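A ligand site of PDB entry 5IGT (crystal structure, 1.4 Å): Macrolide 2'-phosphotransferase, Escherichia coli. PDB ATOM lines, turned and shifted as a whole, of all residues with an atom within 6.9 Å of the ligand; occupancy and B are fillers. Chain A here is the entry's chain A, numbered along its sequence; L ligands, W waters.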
ATOM      1  N   ASN A  30      25.698   6.721 -16.702  1.00  0.00           N
ATOM      2  CA  ASN A  30      26.316   5.635 -17.424  1.00  0.00           C
ATOM      3  C   ASN A  30      25.300   5.058 -18.386  1.00  0.00           C
ATOM      4  O   ASN A  30      24.295   4.455 -17.956  1.00  0.00           O
ATOM      5  CB  ASN A  30      26.818   4.578 -16.449  1.00  0.00           C
ATOM      6  CG  ASN A  30      27.592   3.476 -17.130  1.00  0.00           C
ATOM      7  OD1 ASN A  30      27.383   3.202 -18.315  1.00  0.00           O
ATOM      8  ND2 ASN A  30      28.476   2.831 -16.385  1.00  0.00           N
ATOM      9  N   ILE A  38      22.073   4.051 -16.023  1.00  0.00           N
ATOM     10  CA  ILE A  38      22.335   4.140 -14.588  1.00  0.00           C
ATOM     11  C   ILE A  38      22.779   5.546 -14.291  1.00  0.00           C
ATOM     12  O   ILE A  38      23.751   6.050 -14.859  1.00  0.00           O
ATOM     13  CB  ILE A  38      23.442   3.161 -14.133  1.00  0.00           C
ATOM     14  CG1 ILE A  38      23.097   1.721 -14.567  1.00  0.00           C
ATOM     15  CG2 ILE A  38      23.643   3.239 -12.638  1.00  0.00           C
ATOM     16  CD1 ILE A  38      21.881   1.148 -13.913  1.00  0.00           C
ATOM     17  N   ILE A  40      23.676   8.254 -11.137  1.00  0.00           N
ATOM     18  CA  ILE A  40      23.812   8.560  -9.714  1.00  0.00           C
ATOM     19  C   ILE A  40      23.525  10.036  -9.534  1.00  0.00           C
ATOM     20  O   ILE A  40      24.212  10.890 -10.133  1.00  0.00           O
ATOM     21  CB  ILE A  40      25.192   8.209  -9.195  1.00  0.00           C
ATOM     22  CG1 ILE A  40      25.407   6.694  -9.366  1.00  0.00           C
ATOM     23  CG2 ILE A  40      25.294   8.627  -7.735  1.00  0.00           C
ATOM     24  CD1 ILE A  40      26.745   6.206  -8.836  1.00  0.00           C
ATOM     25  N   ARG A  48      22.876  10.892  -2.131  1.00  0.00           N
ATOM     26  CA  ARG A  48      22.935  10.377  -3.484  1.00  0.00           C
ATOM     27  C   ARG A  48      22.071   9.125  -3.617  1.00  0.00           C
ATOM     28  O   ARG A  48      22.028   8.287  -2.716  1.00  0.00           O
ATOM     29  CB  ARG A  48      24.357  10.054  -3.834  1.00  0.00           C
ATOM     30  CG  ARG A  48      25.239  11.292  -3.851  1.00  0.00           C
ATOM     31  CD  ARG A  48      26.292  11.148  -4.872  1.00  0.00           C
ATOM     32  NE  ARG A  48      27.227  10.114  -4.492  1.00  0.00           N
ATOM     33  CZ  ARG A  48      28.222   9.687  -5.264  1.00  0.00           C
ATOM     34  NH1 ARG A  48      28.416  10.208  -6.464  1.00  0.00           N
ATOM     35  NH2 ARG A  48      29.024   8.727  -4.825  1.00  0.00           N
ATOM     36  N   VAL A  50      20.856   6.037  -6.581  1.00  0.00           N
ATOM     37  CA  VAL A  50      21.067   5.371  -7.853  1.00  0.00           C
ATOM     38  C   VAL A  50      19.720   5.255  -8.561  1.00  0.00           C
ATOM     39  O   VAL A  50      18.771   4.739  -7.975  1.00  0.00           O
ATOM     40  CB  VAL A  50      21.690   3.992  -7.632  1.00  0.00           C
ATOM     41  CG1 VAL A  50      21.895   3.304  -8.995  1.00  0.00           C
ATOM     42  CG2 VAL A  50      23.019   4.119  -6.888  1.00  0.00           C
ATOM     43  N   ARG A  52      18.123   3.460 -11.643  1.00  0.00           N
ATOM     44  CA  ARG A  52      18.321   2.328 -12.533  1.00  0.00           C
ATOM     45  C   ARG A  52      17.118   2.334 -13.476  1.00  0.00           C
ATOM     46  O   ARG A  52      16.002   2.009 -13.075  1.00  0.00           O
ATOM     47  CB  ARG A  52      18.396   1.094 -11.636  1.00  0.00           C
ATOM     48  CG  ARG A  52      18.508  -0.192 -12.305  1.00  0.00           C
ATOM     49  CD  ARG A  52      18.689  -1.264 -11.209  1.00  0.00           C
ATOM     50  NE  ARG A  52      18.899  -2.568 -11.809  1.00  0.00           N
ATOM     51  CZ  ARG A  52      20.053  -2.986 -12.294  1.00  0.00           C
ATOM     52  NH1 ARG A  52      21.132  -2.209 -12.233  1.00  0.00           N
ATOM     53  NH2 ARG A  52      20.147  -4.191 -12.845  1.00  0.00           N
ATOM     54  N   PRO A  82      21.053  -3.192  -2.197  1.00  0.00           N
ATOM     55  CA  PRO A  82      20.236  -2.029  -2.578  1.00  0.00           C
ATOM     56  C   PRO A  82      18.829  -2.098  -1.986  1.00  0.00           C
ATOM     57  O   PRO A  82      18.178  -3.156  -2.013  1.00  0.00           O
ATOM     58  CB  PRO A  82      20.206  -2.123  -4.112  1.00  0.00           C
ATOM     59  CG  PRO A  82      21.520  -2.797  -4.466  1.00  0.00           C
ATOM     60  CD  PRO A  82      21.682  -3.836  -3.369  1.00  0.00           C
ATOM     61  N   TYR A  94      17.267   3.617  -5.526  1.00  0.00           N
ATOM     62  CA  TYR A  94      17.710   3.262  -4.185  1.00  0.00           C
ATOM     63  C   TYR A  94      18.741   4.256  -3.690  1.00  0.00           C
ATOM     64  O   TYR A  94      19.530   4.788  -4.485  1.00  0.00           O
ATOM     65  CB  TYR A  94      18.227   1.836  -4.118  1.00  0.00           C
ATOM     66  CG  TYR A  94      19.367   1.429  -5.046  1.00  0.00           C
ATOM     67  CD1 TYR A  94      19.113   0.916  -6.309  1.00  0.00           C
ATOM     68  CD2 TYR A  94      20.675   1.492  -4.630  1.00  0.00           C
ATOM     69  CE1 TYR A  94      20.131   0.476  -7.137  1.00  0.00           C
ATOM     70  CE2 TYR A  94      21.721   1.059  -5.461  1.00  0.00           C
ATOM     71  CZ  TYR A  94      21.426   0.546  -6.704  1.00  0.00           C
ATOM     72  OH  TYR A  94      22.431   0.078  -7.541  1.00  0.00           O
ATOM     73  N   PRO A  95      18.766   4.508  -2.380  1.00  0.00           N
ATOM     74  CA  PRO A  95      19.849   5.337  -1.847  1.00  0.00           C
ATOM     75  C   PRO A  95      21.186   4.708  -2.160  1.00  0.00           C
ATOM     76  O   PRO A  95      21.350   3.501  -2.026  1.00  0.00           O
ATOM     77  CB  PRO A  95      19.614   5.325  -0.330  1.00  0.00           C
ATOM     78  CG  PRO A  95      18.287   4.725  -0.105  1.00  0.00           C
ATOM     79  CD  PRO A  95      17.831   4.027  -1.348  1.00  0.00           C
ATOM     80  N   MET A  96      22.152   5.480  -2.625  1.00  0.00           N
ATOM     81  CA  MET A  96      23.425   4.896  -2.993  1.00  0.00           C
ATOM     82  C   MET A  96      24.104   4.317  -1.768  1.00  0.00           C
ATOM     83  O   MET A  96      24.119   4.923  -0.702  1.00  0.00           O
ATOM     84  CB  MET A  96      24.341   5.908  -3.664  1.00  0.00           C
ATOM     85  CG  MET A  96      25.633   5.265  -4.184  1.00  0.00           C
ATOM     86  SD  MET A  96      26.784   6.479  -4.839  1.00  0.00           S
ATOM     87  CE  MET A  96      28.183   5.460  -5.264  1.00  0.00           C
ATOM     88  N   LEU A  97      24.672   3.132  -1.924  1.00  0.00           N
ATOM     89  CA  LEU A  97      25.523   2.522  -0.912  1.00  0.00           C
ATOM     90  C   LEU A  97      26.905   3.114  -1.174  1.00  0.00           C
ATOM     91  O   LEU A  97      27.539   2.847  -2.206  1.00  0.00           O
ATOM     92  CB  LEU A  97      25.515   0.994  -1.041  1.00  0.00           C
ATOM     93  CG  LEU A  97      24.128   0.357  -0.908  1.00  0.00           C
ATOM     94  CD1 LEU A  97      24.181  -1.140  -1.205  1.00  0.00           C
ATOM     95  CD2 LEU A  97      23.558   0.561   0.472  1.00  0.00           C
ATOM     96  N   GLU A  98      27.356   3.990  -0.304  1.00  0.00           N
ATOM     97  CA  GLU A  98      28.471   4.853  -0.674  1.00  0.00           C
ATOM     98  C   GLU A  98      29.817   4.169  -0.602  1.00  0.00           C
ATOM     99  O   GLU A  98      30.800   4.690  -1.138  1.00  0.00           O
ATOM    100  CB  GLU A  98      28.461   6.143   0.155  1.00  0.00           C
ATOM    101  CG  GLU A  98      27.311   7.089  -0.222  1.00  0.00           C
ATOM    102  CD  GLU A  98      27.546   7.825  -1.549  1.00  0.00           C
ATOM    103  OE1 GLU A  98      28.560   7.572  -2.240  1.00  0.00           O
ATOM    104  OE2 GLU A  98      26.680   8.650  -1.911  1.00  0.00           O
ATOM    105  N   ASP A  99      29.887   3.001   0.024  1.00  0.00           N
ATOM    106  CA  ASP A  99      31.149   2.271   0.061  1.00  0.00           C
ATOM    107  C   ASP A  99      31.571   1.942  -1.367  1.00  0.00           C
ATOM    108  O   ASP A  99      30.748   1.648  -2.231  1.00  0.00           O
ATOM    109  CB  ASP A  99      31.019   0.988   0.885  1.00  0.00           C
ATOM    110  CG  ASP A  99      31.072   1.205   2.374  1.00  0.00           C
ATOM    111  OD1 ASP A  99      31.289   2.361   2.800  1.00  0.00           O
ATOM    112  OD2 ASP A  99      30.938   0.208   3.110  1.00  0.00           O
ATOM    113  N   SER A 100      32.857   1.913  -1.609  1.00  0.00           N
ATOM    114  CA  SER A 100      33.407   1.630  -2.918  1.00  0.00           C
ATOM    115  C   SER A 100      33.155   0.185  -3.319  1.00  0.00           C
ATOM    116  O   SER A 100      33.113  -0.701  -2.463  1.00  0.00           O
ATOM    117  CB  SER A 100      34.922   1.823  -2.878  1.00  0.00           C
ATOM    118  OG  SER A 100      35.518   1.652  -4.174  1.00  0.00           O
ATOM    119  N   THR A 101      33.029  -0.068  -4.612  1.00  0.00           N
ATOM    120  CA  THR A 101      33.215  -1.403  -5.151  1.00  0.00           C
ATOM    121  C   THR A 101      34.671  -1.870  -4.908  1.00  0.00           C
ATOM    122  O   THR A 101      35.581  -1.043  -4.719  1.00  0.00           O
ATOM    123  CB  THR A 101      32.823  -1.445  -6.657  1.00  0.00           C
ATOM    124  OG1 THR A 101      33.500  -0.381  -7.343  1.00  0.00           O
ATOM    125  CG2 THR A 101      31.326  -1.262  -6.814  1.00  0.00           C
ATOM    126  N   MET A 103      36.572  -3.073  -6.942  1.00  0.00           N
ATOM    127  CA  MET A 103      37.411  -2.700  -8.043  1.00  0.00           C
ATOM    128  C   MET A 103      36.811  -1.455  -8.623  1.00  0.00           C
ATOM    129  O   MET A 103      35.595  -1.230  -8.592  1.00  0.00           O
ATOM    130  CB  MET A 103      37.428  -3.803  -9.055  1.00  0.00           C
ATOM    131  CG  MET A 103      36.064  -4.168  -9.510  1.00  0.00           C
ATOM    132  SD  MET A 103      35.985  -4.535 -11.243  1.00  0.00           S
ATOM    133  CE  MET A 103      36.666  -3.005 -11.927  1.00  0.00           C
ATOM    134  N   ILE A 105      36.808   1.050 -12.021  1.00  0.00           N
ATOM    135  CA  ILE A 105      37.070   1.117 -13.456  1.00  0.00           C
ATOM    136  C   ILE A 105      36.338   2.309 -14.050  1.00  0.00           C
ATOM    137  O   ILE A 105      35.215   2.639 -13.659  1.00  0.00           O
ATOM    138  CB  ILE A 105      36.683  -0.213 -14.157  1.00  0.00           C
ATOM    139  CG1 ILE A 105      37.157  -0.218 -15.602  1.00  0.00           C
ATOM    140  CG2 ILE A 105      35.178  -0.467 -14.113  1.00  0.00           C
ATOM    141  CD1 ILE A 105      37.157  -1.600 -16.231  1.00  0.00           C
ATOM    142  N   TYR A 202      31.428 -10.823  -8.649  1.00  0.00           N
ATOM    143  CA  TYR A 202      32.872 -10.595  -8.840  1.00  0.00           C
ATOM    144  C   TYR A 202      33.175  -9.309  -8.101  1.00  0.00           C
ATOM    145  O   TYR A 202      32.275  -8.631  -7.594  1.00  0.00           O
ATOM    146  CB  TYR A 202      33.249 -10.524 -10.331  1.00  0.00           C
ATOM    147  CG  TYR A 202      32.946  -9.216 -11.025  1.00  0.00           C
ATOM    148  CD1 TYR A 202      31.651  -8.767 -11.173  1.00  0.00           C
ATOM    149  CD2 TYR A 202      33.972  -8.444 -11.528  1.00  0.00           C
ATOM    150  CE1 TYR A 202      31.394  -7.554 -11.841  1.00  0.00           C
ATOM    151  CE2 TYR A 202      33.723  -7.246 -12.170  1.00  0.00           C
ATOM    152  CZ  TYR A 202      32.445  -6.829 -12.319  1.00  0.00           C
ATOM    153  OH  TYR A 202      32.280  -5.621 -12.985  1.00  0.00           O
ATOM    154  N   GLY A 204      33.686  -6.316  -8.908  1.00  0.00           N
ATOM    155  CA  GLY A 204      32.915  -5.134  -9.291  1.00  0.00           C
ATOM    156  C   GLY A 204      31.503  -5.028  -8.717  1.00  0.00           C
ATOM    157  O   GLY A 204      30.873  -3.963  -8.787  1.00  0.00           O
ATOM    158  N   HIS A 205      30.964  -6.126  -8.179  1.00  0.00           N
ATOM    159  CA  HIS A 205      29.648  -6.107  -7.537  1.00  0.00           C
ATOM    160  C   HIS A 205      29.705  -6.315  -6.043  1.00  0.00           C
ATOM    161  O   HIS A 205      28.688  -6.552  -5.403  1.00  0.00           O
ATOM    162  CB  HIS A 205      28.765  -7.186  -8.191  1.00  0.00           C
ATOM    163  CG  HIS A 205      28.407  -6.868  -9.598  1.00  0.00           C
ATOM    164  ND1 HIS A 205      27.973  -7.822 -10.505  1.00  0.00           N
ATOM    165  CD2 HIS A 205      28.416  -5.698 -10.278  1.00  0.00           C
ATOM    166  CE1 HIS A 205      27.718  -7.247 -11.656  1.00  0.00           C
ATOM    167  NE2 HIS A 205      27.972  -5.958 -11.554  1.00  0.00           N
ATOM    168  N   LEU A 207      30.868  -4.465  -2.452  1.00  0.00           N
ATOM    169  CA  LEU A 207      31.259  -3.240  -1.796  1.00  0.00           C
ATOM    170  C   LEU A 207      32.111  -3.526  -0.574  1.00  0.00           C
ATOM    171  O   LEU A 207      31.906  -4.530   0.115  1.00  0.00           O
ATOM    172  CB  LEU A 207      30.043  -2.435  -1.345  1.00  0.00           C
ATOM    173  CG  LEU A 207      28.998  -2.222  -2.426  1.00  0.00           C
ATOM    174  CD1 LEU A 207      27.901  -1.287  -1.903  1.00  0.00           C
ATOM    175  CD2 LEU A 207      29.597  -1.687  -3.715  1.00  0.00           C
ATOM    176  N   ILE A 218      25.984  -5.632  -4.814  1.00  0.00           N
ATOM    177  CA  ILE A 218      25.035  -4.966  -5.692  1.00  0.00           C
ATOM    178  C   ILE A 218      24.804  -5.799  -6.942  1.00  0.00           C
ATOM    179  O   ILE A 218      25.460  -6.827  -7.142  1.00  0.00           O
ATOM    180  CB  ILE A 218      25.567  -3.565  -6.101  1.00  0.00           C
ATOM    181  CG1 ILE A 218      26.899  -3.686  -6.817  1.00  0.00           C
ATOM    182  CG2 ILE A 218      25.680  -2.656  -4.871  1.00  0.00           C
ATOM    183  CD1 ILE A 218      27.413  -2.381  -7.404  1.00  0.00           C
ATOM    184  N   ASP A 219      23.838  -5.362  -7.747  1.00  0.00           N
ATOM    185  CA  ASP A 219      23.554  -5.905  -9.076  1.00  0.00           C
ATOM    186  C   ASP A 219      23.110  -7.383  -8.987  1.00  0.00           C
ATOM    187  O   ASP A 219      23.804  -8.301  -9.445  1.00  0.00           O
ATOM    188  CB  ASP A 219      24.740  -5.721 -10.031  1.00  0.00           C
ATOM    189  CG  ASP A 219      25.010  -4.245 -10.423  1.00  0.00           C
ATOM    190  OD1 ASP A 219      24.229  -3.350 -10.098  1.00  0.00           O
ATOM    191  OD2 ASP A 219      26.034  -4.012 -11.093  1.00  0.00           O
HETATM  192  O1  LIG L   1      24.630  -0.853 -11.250  1.00  0.00           O
HETATM  193  C1  LIG L   1      25.586  -0.463 -12.242  1.00  0.00           C
HETATM  194  C2  LIG L   1      26.929  -0.062 -11.662  1.00  0.00           C
HETATM  195  O2  LIG L   1      26.824   1.187 -10.934  1.00  0.00           O
HETATM  196  C3  LIG L   1      27.552  -1.025 -10.652  1.00  0.00           C
HETATM  197  O3  LIG L   1      28.193  -2.133 -11.260  1.00  0.00           O
HETATM  198  C4  LIG L   1      28.475  -0.114  -9.858  1.00  0.00           C
HETATM  199  O4  LIG L   1      29.666   0.197 -10.582  1.00  0.00           O
HETATM  200  C5  LIG L   1      27.640   1.148  -9.770  1.00  0.00           C
HETATM  201  N1  LIG L   1      26.745   1.128  -8.601  1.00  0.00           N
HETATM  202  C6  LIG L   1      25.397   0.933  -8.684  1.00  0.00           C
HETATM  203  N2  LIG L   1      24.884   0.989  -7.433  1.00  0.00           N
HETATM  204  C7  LIG L   1      25.910   1.274  -6.549  1.00  0.00           C
HETATM  205  C8  LIG L   1      25.982   1.479  -5.136  1.00  0.00           C
HETATM  206  O5  LIG L   1      24.902   1.462  -4.336  1.00  0.00           O
HETATM  207  N3  LIG L   1      27.197   1.734  -4.554  1.00  0.00           N
HETATM  208  C9  LIG L   1      28.380   1.831  -5.351  1.00  0.00           C
HETATM  209  N4  LIG L   1      29.567   2.092  -4.673  1.00  0.00           N
HETATM  210  N5  LIG L   1      28.347   1.651  -6.737  1.00  0.00           N
HETATM  211  C10 LIG L   1      27.113   1.385  -7.280  1.00  0.00           C
HETATM  212  O   HOH W   1      30.510   2.485  -8.209  1.00  0.00           O
HETATM  213  O   HOH W   2      31.320  -1.984 -10.608  1.00  0.00           O
HETATM  214  O   HOH W   3      32.101   2.586  -6.074  1.00  0.00           O
HETATM  215  O   HOH W   4      21.918  -0.176 -10.501  1.00  0.00           O
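A nitrogen (N3) of the ligand is in hydrogen-bond range of the backbone carbonyl oxygen (O) of Leu 97 (2.6 Å). O1 of the ligand lies within hydrogen-bond range of OD1 of Asp 219 (2.8 Å). N of Leu 97 is in hydrogen-bond range of O5 of the ligand (2.9 Å). A nitrogen (N4) of the ligand lies within hydrogen-bond range of the backbone carbonyl oxygen of Asp 99, at 2.7 Å. A nitrogen (N2) of the ligand is in hydrogen-bond range of the side-chain hydroxyl (OH) of Tyr 94.
Val 50 touches the ligand. Arg 52 touches the ligand. Met 96 touches the ligand (CE to C9, 3.6 Å). CD2 of His 205 touches O3 of the ligand, 3.7 Å away. Leu 207 touches the ligand. Ile 218 touches the ligand. Hydrophobic or aromatic side chains that line the ligand: Val 50, Tyr 94, Met 96, Leu 97, His 205, Leu 207 and Ile 218. Of the 23 residues printed, 10 come within 4 Å of the ligand. The nearest printed residue that does not touch the ligand is Ile 38 (4.05 Å).
The backbone carbonyl oxygen of His 205 sits at hydrogen-bond distance from the backbone NH of Ile 218, at 2.9 Å. O of Tyr 94 lies within hydrogen-bond range of N of Val 50, 2.8 Å away. The side-chain carboxylate of Asp 219 is in hydrogen-bond range of a ring nitrogen (NE2) of His 205 (2.8 Å). The backbone carbonyl oxygen (O) of Arg 48 is in hydrogen-bond range of the backbone NH (N) of Met 96, 2.8 Å away. The side-chain carboxylate of Asp 219 lies within salt-bridge range of the guanidinium group of Arg 52, 3.9 Å away.
Water W2 lies within hydrogen-bond range of O of Gly 204 (2.7 Å) and O4 of the ligand (2.7 Å). Water W4 lies within hydrogen-bond range of the guanidinium group of Arg 52, an oxygen (O1) of the ligand and the side-chain hydroxyl of Tyr 94. Water W3 lies within hydrogen-bond range of N4 of the ligand (2.9 Å) and N of Thr 101 (3.2 Å).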
